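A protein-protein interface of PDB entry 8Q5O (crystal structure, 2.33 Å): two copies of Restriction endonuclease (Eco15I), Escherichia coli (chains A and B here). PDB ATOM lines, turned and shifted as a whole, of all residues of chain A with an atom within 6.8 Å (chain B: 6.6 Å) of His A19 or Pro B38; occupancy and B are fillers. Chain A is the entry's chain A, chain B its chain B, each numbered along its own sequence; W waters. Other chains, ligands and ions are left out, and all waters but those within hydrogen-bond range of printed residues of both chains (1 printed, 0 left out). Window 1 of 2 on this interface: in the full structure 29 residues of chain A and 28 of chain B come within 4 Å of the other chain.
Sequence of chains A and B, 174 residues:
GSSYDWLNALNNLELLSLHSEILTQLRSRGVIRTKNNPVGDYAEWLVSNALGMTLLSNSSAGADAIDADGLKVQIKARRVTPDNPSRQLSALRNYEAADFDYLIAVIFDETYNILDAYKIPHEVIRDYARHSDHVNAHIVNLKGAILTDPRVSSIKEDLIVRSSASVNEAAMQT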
ATOM      1  N   GLU A  14       5.044   2.256   6.271  1.00  0.00           N
ATOM      2  CA  GLU A  14       4.046   1.836   7.238  1.00  0.00           C
ATOM      3  C   GLU A  14       2.639   2.027   6.677  1.00  0.00           C
ATOM      4  O   GLU A  14       1.760   1.202   6.941  1.00  0.00           O
ATOM      5  CB  GLU A  14       4.238   2.618   8.532  1.00  0.00           C
ATOM      6  CG  GLU A  14       5.611   2.399   9.158  1.00  0.00           C
ATOM      7  CD  GLU A  14       5.966   3.417  10.228  1.00  0.00           C
ATOM      8  OE1 GLU A  14       5.136   4.333  10.488  1.00  0.00           O
ATOM      9  OE2 GLU A  14       7.077   3.302  10.790  1.00  0.00           O
ATOM     10  N   LEU A  15       2.430   3.098   5.898  1.00  0.00           N
ATOM     11  CA  LEU A  15       1.131   3.361   5.304  1.00  0.00           C
ATOM     12  C   LEU A  15       0.801   2.251   4.310  1.00  0.00           C
ATOM     13  O   LEU A  15      -0.303   1.713   4.321  1.00  0.00           O
ATOM     14  CB  LEU A  15       1.137   4.720   4.590  1.00  0.00           C
ATOM     15  CG  LEU A  15       1.232   5.976   5.454  1.00  0.00           C
ATOM     16  CD1 LEU A  15       1.335   7.213   4.556  1.00  0.00           C
ATOM     17  CD2 LEU A  15       0.055   6.103   6.401  1.00  0.00           C
ATOM     18  N   SER A  17       2.116  -0.773   4.180  1.00  0.00           N
ATOM     19  CA  SER A  17       2.036  -2.056   4.861  1.00  0.00           C
ATOM     20  C   SER A  17       0.667  -2.203   5.516  1.00  0.00           C
ATOM     21  O   SER A  17       0.052  -3.256   5.443  1.00  0.00           O
ATOM     22  CB  SER A  17       3.140  -2.241   5.850  1.00  0.00           C
ATOM     23  OG  SER A  17       2.705  -1.906   7.154  1.00  0.00           O
ATOM     24  N   LEU A  18       0.099  -1.108   6.003  1.00  0.00           N
ATOM     25  CA  LEU A  18      -1.224  -1.187   6.673  1.00  0.00           C
ATOM     26  C   LEU A  18      -2.329  -1.468   5.647  1.00  0.00           C
ATOM     27  O   LEU A  18      -3.338  -2.090   6.024  1.00  0.00           O
ATOM     28  CB  LEU A  18      -1.497   0.120   7.420  1.00  0.00           C
ATOM     29  CG  LEU A  18      -2.729   0.108   8.322  1.00  0.00           C
ATOM     30  CD1 LEU A  18      -2.423  -0.580   9.642  1.00  0.00           C
ATOM     31  CD2 LEU A  18      -3.243   1.518   8.559  1.00  0.00           C
ATOM     32  N   HIS A  19      -2.146  -0.998   4.412  1.00  0.00           N
ATOM     33  CA  HIS A  19      -3.165  -1.188   3.343  1.00  0.00           C
ATOM     34  C   HIS A  19      -3.155  -2.662   2.963  1.00  0.00           C
ATOM     35  O   HIS A  19      -4.227  -3.226   2.699  1.00  0.00           O
ATOM     36  CB  HIS A  19      -2.871  -0.255   2.167  1.00  0.00           C
ATOM     37  CG  HIS A  19      -3.384  -0.698   0.846  1.00  0.00           C
ATOM     38  ND1 HIS A  19      -4.717  -0.717   0.513  1.00  0.00           N
ATOM     39  CD2 HIS A  19      -2.722  -1.093  -0.243  1.00  0.00           C
ATOM     40  CE1 HIS A  19      -4.845  -1.142  -0.733  1.00  0.00           C
ATOM     41  NE2 HIS A  19      -3.646  -1.374  -1.211  1.00  0.00           N
ATOM     42  N   SER A  20      -1.964  -3.252   2.934  1.00  0.00           N
ATOM     43  CA  SER A  20      -1.856  -4.710   2.686  1.00  0.00           C
ATOM     44  C   SER A  20      -2.599  -5.433   3.804  1.00  0.00           C
ATOM     45  O   SER A  20      -3.307  -6.387   3.503  1.00  0.00           O
ATOM     46  CB  SER A  20      -0.431  -5.149   2.623  1.00  0.00           C
ATOM     47  OG  SER A  20      -0.323  -6.546   2.827  1.00  0.00           O
ATOM     48  N   GLU A  21      -2.410  -4.995   5.048  1.00  0.00           N
ATOM     49  CA  GLU A  21      -3.045  -5.680   6.201  1.00  0.00           C
ATOM     50  C   GLU A  21      -4.566  -5.580   6.066  1.00  0.00           C
ATOM     51  O   GLU A  21      -5.257  -6.541   6.420  1.00  0.00           O
ATOM     52  CB  GLU A  21      -2.560  -5.064   7.510  1.00  0.00           C
ATOM     53  CG  GLU A  21      -2.851  -5.923   8.724  1.00  0.00           C
ATOM     54  CD  GLU A  21      -2.432  -7.373   8.566  1.00  0.00           C
ATOM     55  OE1 GLU A  21      -3.302  -8.255   8.696  1.00  0.00           O
ATOM     56  OE2 GLU A  21      -1.237  -7.613   8.302  1.00  0.00           O
ATOM     57  N   ILE A  22      -5.069  -4.452   5.577  1.00  0.00           N
ATOM     58  CA  ILE A  22      -6.541  -4.290   5.518  1.00  0.00           C
ATOM     59  C   ILE A  22      -7.053  -5.267   4.469  1.00  0.00           C
ATOM     60  O   ILE A  22      -8.128  -5.821   4.665  1.00  0.00           O
ATOM     61  CB  ILE A  22      -6.926  -2.835   5.196  1.00  0.00           C
ATOM     62  N   LEU A  23      -6.296  -5.419   3.387  1.00  0.00           N
ATOM     63  CA  LEU A  23      -6.698  -6.356   2.311  1.00  0.00           C
ATOM     64  C   LEU A  23      -6.720  -7.752   2.927  1.00  0.00           C
ATOM     65  O   LEU A  23      -7.695  -8.481   2.686  1.00  0.00           O
ATOM     66  CB  LEU A  23      -5.701  -6.254   1.155  1.00  0.00           C
ATOM     67  CG  LEU A  23      -5.949  -5.121   0.164  1.00  0.00           C
ATOM     68  CD1 LEU A  23      -5.028  -5.250  -1.038  1.00  0.00           C
ATOM     69  CD2 LEU A  23      -7.400  -5.114  -0.281  1.00  0.00           C
ATOM     70  N   THR A  24      -5.710  -8.069   3.741  1.00  0.00           N
ATOM     71  CA  THR A  24      -5.648  -9.388   4.419  1.00  0.00           C
ATOM     72  C   THR A  24      -6.926  -9.592   5.235  1.00  0.00           C
ATOM     73  O   THR A  24      -7.539 -10.662   5.111  1.00  0.00           O
ATOM     74  CB  THR A  24      -4.409  -9.501   5.315  1.00  0.00           C
ATOM     75  OG1 THR A  24      -4.620  -8.731   6.497  1.00  0.00           O
ATOM     76  CG2 THR A  24      -3.140  -9.049   4.628  1.00  0.00           C
ATOM     77  N   ASN A  36      -6.610  -7.511  -5.710  1.00  0.00           N
ATOM     78  CA  ASN A  36      -6.805  -6.553  -6.777  1.00  0.00           C
ATOM     79  C   ASN A  36      -7.330  -5.264  -6.167  1.00  0.00           C
ATOM     80  O   ASN A  36      -7.181  -5.028  -4.956  1.00  0.00           O
ATOM     81  CB  ASN A  36      -7.813  -7.067  -7.811  1.00  0.00           C
ATOM     82  CG  ASN A  36      -7.173  -7.557  -9.088  1.00  0.00           C
ATOM     83  OD1 ASN A  36      -5.978  -7.392  -9.308  1.00  0.00           O
ATOM     84  ND2 ASN A  36      -7.972  -8.132  -9.960  1.00  0.00           N
ATOM     85  N   PRO A  38      -9.887  -3.275  -4.418  1.00  0.00           N
ATOM     86  CA  PRO A  38     -10.912  -3.763  -3.513  1.00  0.00           C
ATOM     87  C   PRO A  38     -12.352  -3.445  -3.899  1.00  0.00           C
ATOM     88  O   PRO A  38     -13.243  -4.171  -3.454  1.00  0.00           O
ATOM     89  CB  PRO A  38     -10.566  -3.086  -2.173  1.00  0.00           C
ATOM     90  CG  PRO A  38      -9.097  -2.727  -2.292  1.00  0.00           C
ATOM     91  CD  PRO A  38      -8.934  -2.373  -3.750  1.00  0.00           C
ATOM     92  N   HIS B  19      -8.998   2.265   3.519  1.00  0.00           N
ATOM     93  CA  HIS B  19      -8.130   1.951   2.398  1.00  0.00           C
ATOM     94  C   HIS B  19      -7.976   3.172   1.494  1.00  0.00           C
ATOM     95  O   HIS B  19      -6.871   3.607   1.187  1.00  0.00           O
ATOM     96  CB  HIS B  19      -8.705   0.793   1.577  1.00  0.00           C
ATOM     97  CG  HIS B  19      -8.219   0.783   0.174  1.00  0.00           C
ATOM     98  ND1 HIS B  19      -9.086   0.856  -0.890  1.00  0.00           N
ATOM     99  CD2 HIS B  19      -6.996   0.688  -0.354  1.00  0.00           C
ATOM    100  CE1 HIS B  19      -8.390   0.853  -2.016  1.00  0.00           C
ATOM    101  NE2 HIS B  19      -7.120   0.716  -1.717  1.00  0.00           N
ATOM    102  N   SER B  20      -9.112   3.676   1.015  1.00  0.00           N
ATOM    103  CA  SER B  20      -9.094   4.816   0.066  1.00  0.00           C
ATOM    104  C   SER B  20      -8.430   6.020   0.726  1.00  0.00           C
ATOM    105  O   SER B  20      -7.678   6.730   0.051  1.00  0.00           O
ATOM    106  CB  SER B  20     -10.483   5.151  -0.389  1.00  0.00           C
ATOM    107  OG  SER B  20     -10.471   6.269  -1.260  1.00  0.00           O
ATOM    108  N   ILE B  22      -6.113   6.000   3.062  1.00  0.00           N
ATOM    109  CA  ILE B  22      -4.671   5.784   3.083  1.00  0.00           C
ATOM    110  C   ILE B  22      -4.087   6.100   1.706  1.00  0.00           C
ATOM    111  O   ILE B  22      -3.010   6.686   1.601  1.00  0.00           O
ATOM    112  CB  ILE B  22      -4.347   4.351   3.557  1.00  0.00           C
ATOM    113  CG1 ILE B  22      -4.411   4.267   5.086  1.00  0.00           C
ATOM    114  CG2 ILE B  22      -3.010   3.855   3.028  1.00  0.00           C
ATOM    115  CD1 ILE B  22      -4.873   2.935   5.605  1.00  0.00           C
ATOM    116  N   LEU B  23      -4.804   5.704   0.650  1.00  0.00           N
ATOM    117  CA  LEU B  23      -4.381   6.011  -0.710  1.00  0.00           C
ATOM    118  C   LEU B  23      -4.288   7.520  -0.901  1.00  0.00           C
ATOM    119  O   LEU B  23      -3.389   8.004  -1.571  1.00  0.00           O
ATOM    120  CB  LEU B  23      -5.355   5.416  -1.739  1.00  0.00           C
ATOM    121  CG  LEU B  23      -5.402   3.900  -1.819  1.00  0.00           C
ATOM    122  CD1 LEU B  23      -5.866   3.490  -3.203  1.00  0.00           C
ATOM    123  CD2 LEU B  23      -4.051   3.300  -1.490  1.00  0.00           C
ATOM    124  N   LEU B  26      -0.934   8.944   0.628  1.00  0.00           N
ATOM    125  CA  LEU B  26       0.264   8.739  -0.172  1.00  0.00           C
ATOM    126  C   LEU B  26       0.208   9.625  -1.413  1.00  0.00           C
ATOM    127  O   LEU B  26       1.242  10.091  -1.860  1.00  0.00           O
ATOM    128  CB  LEU B  26       0.368   7.271  -0.586  1.00  0.00           C
ATOM    129  CG  LEU B  26       1.070   6.342   0.412  1.00  0.00           C
ATOM    130  CD1 LEU B  26       0.064   5.784   1.390  1.00  0.00           C
ATOM    131  CD2 LEU B  26       1.764   5.202  -0.310  1.00  0.00           C
ATOM    132  N   VAL B  31       3.485  10.118  -3.286  1.00  0.00           N
ATOM    133  CA  VAL B  31       3.983   8.749  -3.439  1.00  0.00           C
ATOM    134  C   VAL B  31       3.310   8.091  -4.630  1.00  0.00           C
ATOM    135  O   VAL B  31       3.934   7.365  -5.387  1.00  0.00           O
ATOM    136  CB  VAL B  31       3.763   7.936  -2.150  1.00  0.00           C
ATOM    137  CG1 VAL B  31       4.518   6.614  -2.175  1.00  0.00           C
ATOM    138  CG2 VAL B  31       4.134   8.754  -0.913  1.00  0.00           C
ATOM    139  N   ILE B  32       2.015   8.356  -4.807  1.00  0.00           N
ATOM    140  CA  ILE B  32       1.254   7.778  -5.903  1.00  0.00           C
ATOM    141  C   ILE B  32       0.573   8.879  -6.727  1.00  0.00           C
ATOM    142  O   ILE B  32       0.307   9.960  -6.226  1.00  0.00           O
ATOM    143  CB  ILE B  32       0.219   6.782  -5.357  1.00  0.00           C
ATOM    144  CG1 ILE B  32      -0.578   7.391  -4.207  1.00  0.00           C
ATOM    145  CG2 ILE B  32       0.908   5.477  -4.960  1.00  0.00           C
ATOM    146  CD1 ILE B  32      -2.018   6.959  -4.186  1.00  0.00           C
ATOM    147  N   THR B  34      -2.383   7.933  -8.754  1.00  0.00           N
ATOM    148  CA  THR B  34      -3.726   7.444  -9.157  1.00  0.00           C
ATOM    149  C   THR B  34      -4.507   6.788  -8.025  1.00  0.00           C
ATOM    150  O   THR B  34      -4.001   6.737  -6.901  1.00  0.00           O
ATOM    151  CB  THR B  34      -3.607   6.330 -10.198  1.00  0.00           C
ATOM    152  OG1 THR B  34      -4.918   5.906 -10.564  1.00  0.00           O
ATOM    153  CG2 THR B  34      -2.833   5.135  -9.690  1.00  0.00           C
ATOM    154  N   LYS B  35      -5.732   6.363  -8.332  1.00  0.00           N
ATOM    155  CA  LYS B  35      -6.564   5.627  -7.353  1.00  0.00           C
ATOM    156  C   LYS B  35      -6.477   4.140  -7.724  1.00  0.00           C
ATOM    157  O   LYS B  35      -7.368   3.373  -7.312  1.00  0.00           O
ATOM    158  CB  LYS B  35      -7.990   6.177  -7.362  1.00  0.00           C
ATOM    159  N   ASN B  36      -5.439   3.757  -8.474  1.00  0.00           N
ATOM    160  CA  ASN B  36      -5.213   2.341  -8.839  1.00  0.00           C
ATOM    161  C   ASN B  36      -4.407   1.642  -7.736  1.00  0.00           C
ATOM    162  O   ASN B  36      -4.488   2.085  -6.579  1.00  0.00           O
ATOM    163  CB  ASN B  36      -4.509   2.272 -10.166  1.00  0.00           C
ATOM    164  N   ASN B  37      -3.659   0.592  -8.086  1.00  0.00           N
ATOM    165  CA  ASN B  37      -2.869  -0.198  -7.103  1.00  0.00           C
ATOM    166  C   ASN B  37      -1.668   0.600  -6.607  1.00  0.00           C
ATOM    167  O   ASN B  37      -0.859   1.020  -7.445  1.00  0.00           O
ATOM    168  CB  ASN B  37      -2.349  -1.482  -7.741  1.00  0.00           C
ATOM    169  CG  ASN B  37      -2.389  -2.679  -6.819  1.00  0.00           C
ATOM    170  OD1 ASN B  37      -1.806  -2.654  -5.740  1.00  0.00           O
ATOM    171  ND2 ASN B  37      -3.069  -3.733  -7.240  1.00  0.00           N
ATOM    172  N   PRO B  38      -1.498   0.791  -5.289  1.00  0.00           N
ATOM    173  CA  PRO B  38      -0.413   1.617  -4.777  1.00  0.00           C
ATOM    174  C   PRO B  38       0.962   1.075  -5.178  1.00  0.00           C
ATOM    175  O   PRO B  38       1.885   1.835  -5.233  1.00  0.00           O
ATOM    176  CB  PRO B  38      -0.560   1.469  -3.262  1.00  0.00           C
ATOM    177  CG  PRO B  38      -1.993   1.058  -3.040  1.00  0.00           C
ATOM    178  CD  PRO B  38      -2.346   0.221  -4.247  1.00  0.00           C
ATOM    179  N   VAL B  39       1.043  -0.214  -5.473  1.00  0.00           N
ATOM    180  CA  VAL B  39       2.336  -0.886  -5.800  1.00  0.00           C
ATOM    181  C   VAL B  39       2.992  -0.269  -7.040  1.00  0.00           C
ATOM    182  O   VAL B  39       4.192   0.009  -6.987  1.00  0.00           O
ATOM    183  CB  VAL B  39       2.105  -2.399  -5.997  1.00  0.00           C
ATOM    184  CG1 VAL B  39       2.094  -3.167  -4.690  1.00  0.00           C
ATOM    185  CG2 VAL B  39       0.843  -2.684  -6.795  1.00  0.00           C
ATOM    186  N   GLY B  40       2.231  -0.076  -8.114  1.00  0.00           N
ATOM    187  CA  GLY B  40       2.811   0.398  -9.385  1.00  0.00           C
ATOM    188  C   GLY B  40       3.364   1.801  -9.286  1.00  0.00           C
ATOM    189  O   GLY B  40       4.478   2.031  -9.767  1.00  0.00           O
ATOM    190  N   ASP B  41       2.593   2.700  -8.682  1.00  0.00           N
ATOM    191  CA  ASP B  41       3.046   4.085  -8.601  1.00  0.00           C
ATOM    192  C   ASP B  41       4.081   4.206  -7.498  1.00  0.00           C
ATOM    193  O   ASP B  41       4.977   5.039  -7.589  1.00  0.00           O
ATOM    194  CB  ASP B  41       1.908   5.066  -8.351  1.00  0.00           C
ATOM    195  CG  ASP B  41       1.094   5.349  -9.587  1.00  0.00           C
ATOM    196  OD1 ASP B  41       1.591   5.165 -10.733  1.00  0.00           O
ATOM    197  OD2 ASP B  41      -0.067   5.716  -9.391  1.00  0.00           O
ATOM    198  N   TYR B  42       3.971   3.363  -6.462  1.00  0.00           N
ATOM    199  CA  TYR B  42       4.993   3.323  -5.430  1.00  0.00           C
ATOM    200  C   TYR B  42       6.300   2.806  -6.014  1.00  0.00           C
ATOM    201  O   TYR B  42       7.378   3.306  -5.687  1.00  0.00           O
ATOM    202  CB  TYR B  42       4.536   2.489  -4.233  1.00  0.00           C
ATOM    203  CG  TYR B  42       5.655   2.142  -3.288  1.00  0.00           C
ATOM    204  CD1 TYR B  42       6.312   3.123  -2.558  1.00  0.00           C
ATOM    205  CD2 TYR B  42       6.116   0.838  -3.191  1.00  0.00           C
ATOM    206  CE1 TYR B  42       7.369   2.805  -1.716  1.00  0.00           C
ATOM    207  CE2 TYR B  42       7.168   0.510  -2.356  1.00  0.00           C
ATOM    208  CZ  TYR B  42       7.794   1.498  -1.618  1.00  0.00           C
ATOM    209  OH  TYR B  42       8.846   1.170  -0.816  1.00  0.00           O
ATOM    210  N   ALA B  43       6.213   1.815  -6.891  1.00  0.00           N
ATOM    211  CA  ALA B  43       7.389   1.343  -7.604  1.00  0.00           C
ATOM    212  C   ALA B  43       7.970   2.479  -8.448  1.00  0.00           C
ATOM    213  O   ALA B  43       9.127   2.846  -8.274  1.00  0.00           O
ATOM    214  CB  ALA B  43       7.065   0.081  -8.416  1.00  0.00           C
ATOM    215  N   ARG B  79       3.568  -7.802  -6.903  1.00  0.00           N
ATOM    216  CA  ARG B  79       3.695  -8.304  -5.511  1.00  0.00           C
ATOM    217  C   ARG B  79       3.355  -9.793  -5.492  1.00  0.00           C
ATOM    218  O   ARG B  79       2.161 -10.127  -5.404  1.00  0.00           O
ATOM    219  CB  ARG B  79       2.745  -7.564  -4.566  1.00  0.00           C
ATOM    220  CG  ARG B  79       3.021  -7.830  -3.094  1.00  0.00           C
ATOM    221  CD  ARG B  79       1.766  -7.789  -2.246  1.00  0.00           C
ATOM    222  NE  ARG B  79       0.930  -6.631  -2.523  1.00  0.00           N
ATOM    223  CZ  ARG B  79      -0.205  -6.357  -1.891  1.00  0.00           C
ATOM    224  NH1 ARG B  79      -0.446  -6.893  -0.708  1.00  0.00           N
ATOM    225  NH2 ARG B  79      -1.091  -5.547  -2.441  1.00  0.00           N
ATOM    226  N   TYR B 112       5.328  -4.856   0.854  1.00  0.00           N
ATOM    227  CA  TYR B 112       5.949  -3.881  -0.040  1.00  0.00           C
ATOM    228  C   TYR B 112       7.460  -3.823   0.186  1.00  0.00           C
ATOM    229  O   TYR B 112       8.016  -2.750   0.456  1.00  0.00           O
ATOM    230  CB  TYR B 112       5.313  -2.504   0.141  1.00  0.00           C
ATOM    231  CG  TYR B 112       3.854  -2.436  -0.235  1.00  0.00           C
ATOM    232  CD1 TYR B 112       2.859  -2.715   0.687  1.00  0.00           C
ATOM    233  CD2 TYR B 112       3.469  -2.045  -1.501  1.00  0.00           C
ATOM    234  CE1 TYR B 112       1.518  -2.646   0.347  1.00  0.00           C
ATOM    235  CE2 TYR B 112       2.136  -1.957  -1.858  1.00  0.00           C
ATOM    236  CZ  TYR B 112       1.153  -2.256  -0.931  1.00  0.00           C
ATOM    237  OH  TYR B 112      -0.184  -2.194  -1.270  1.00  0.00           O
HETATM  238  O   HOH W   1      -3.485  -3.027  -3.551  1.00  0.00           O
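The backbone NH (N) of Val B31 is in hydrogen-bond range of the backbone carbonyl oxygen (O) of Leu B26, at 2.7 Å.
Among the printed residues, pairs that only touch across the chains: Leu A15 with Ile B22, Leu A15 with Leu B26, Leu A18 with Ile B22, His A19 with His B19, His A19 with Pro B38, His A19 with Tyr B112, Ser A20 with Arg B79, Ser A20 with Tyr B112 and Pro A38 with His B19.
Printed residues of chain B within 4 Å of Leu A18: Ile B22 (3.7 Å).
Of the printed residues of chain B, Pro A38 touches His B19.
Pro B38 touches just one residue of chain A: His A19.
Tyr B42 touches none of the printed residues of chain A.
Printed residues of chain A that touch a printed residue of chain B: Leu A15, Leu A18, His A19, Ser A20 and Pro A38.
Hydrophobic or aromatic side chains of chain A that line the printed part of chain B: Leu A15, Leu A18, His A19 and Pro A38.
Of the 19 printed residues of chain B, 6 touch a printed residue of chain A.
Hydrophobic or aromatic side chains of chain B within 4 Å of the printed part of chain A: His B19, Ile B22, Leu B26, Pro B38 and Tyr B112.
His B19 touches its own counterpart, His A19.
His A19 touches Pro B38, and with the chains exchanged Pro A38 touches His B19.
Water W1 bridges the side-chain amide oxygen of Asn B37 (2.8 Å) and a ring nitrogen (NE2) of His A19 (2.9 Å).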
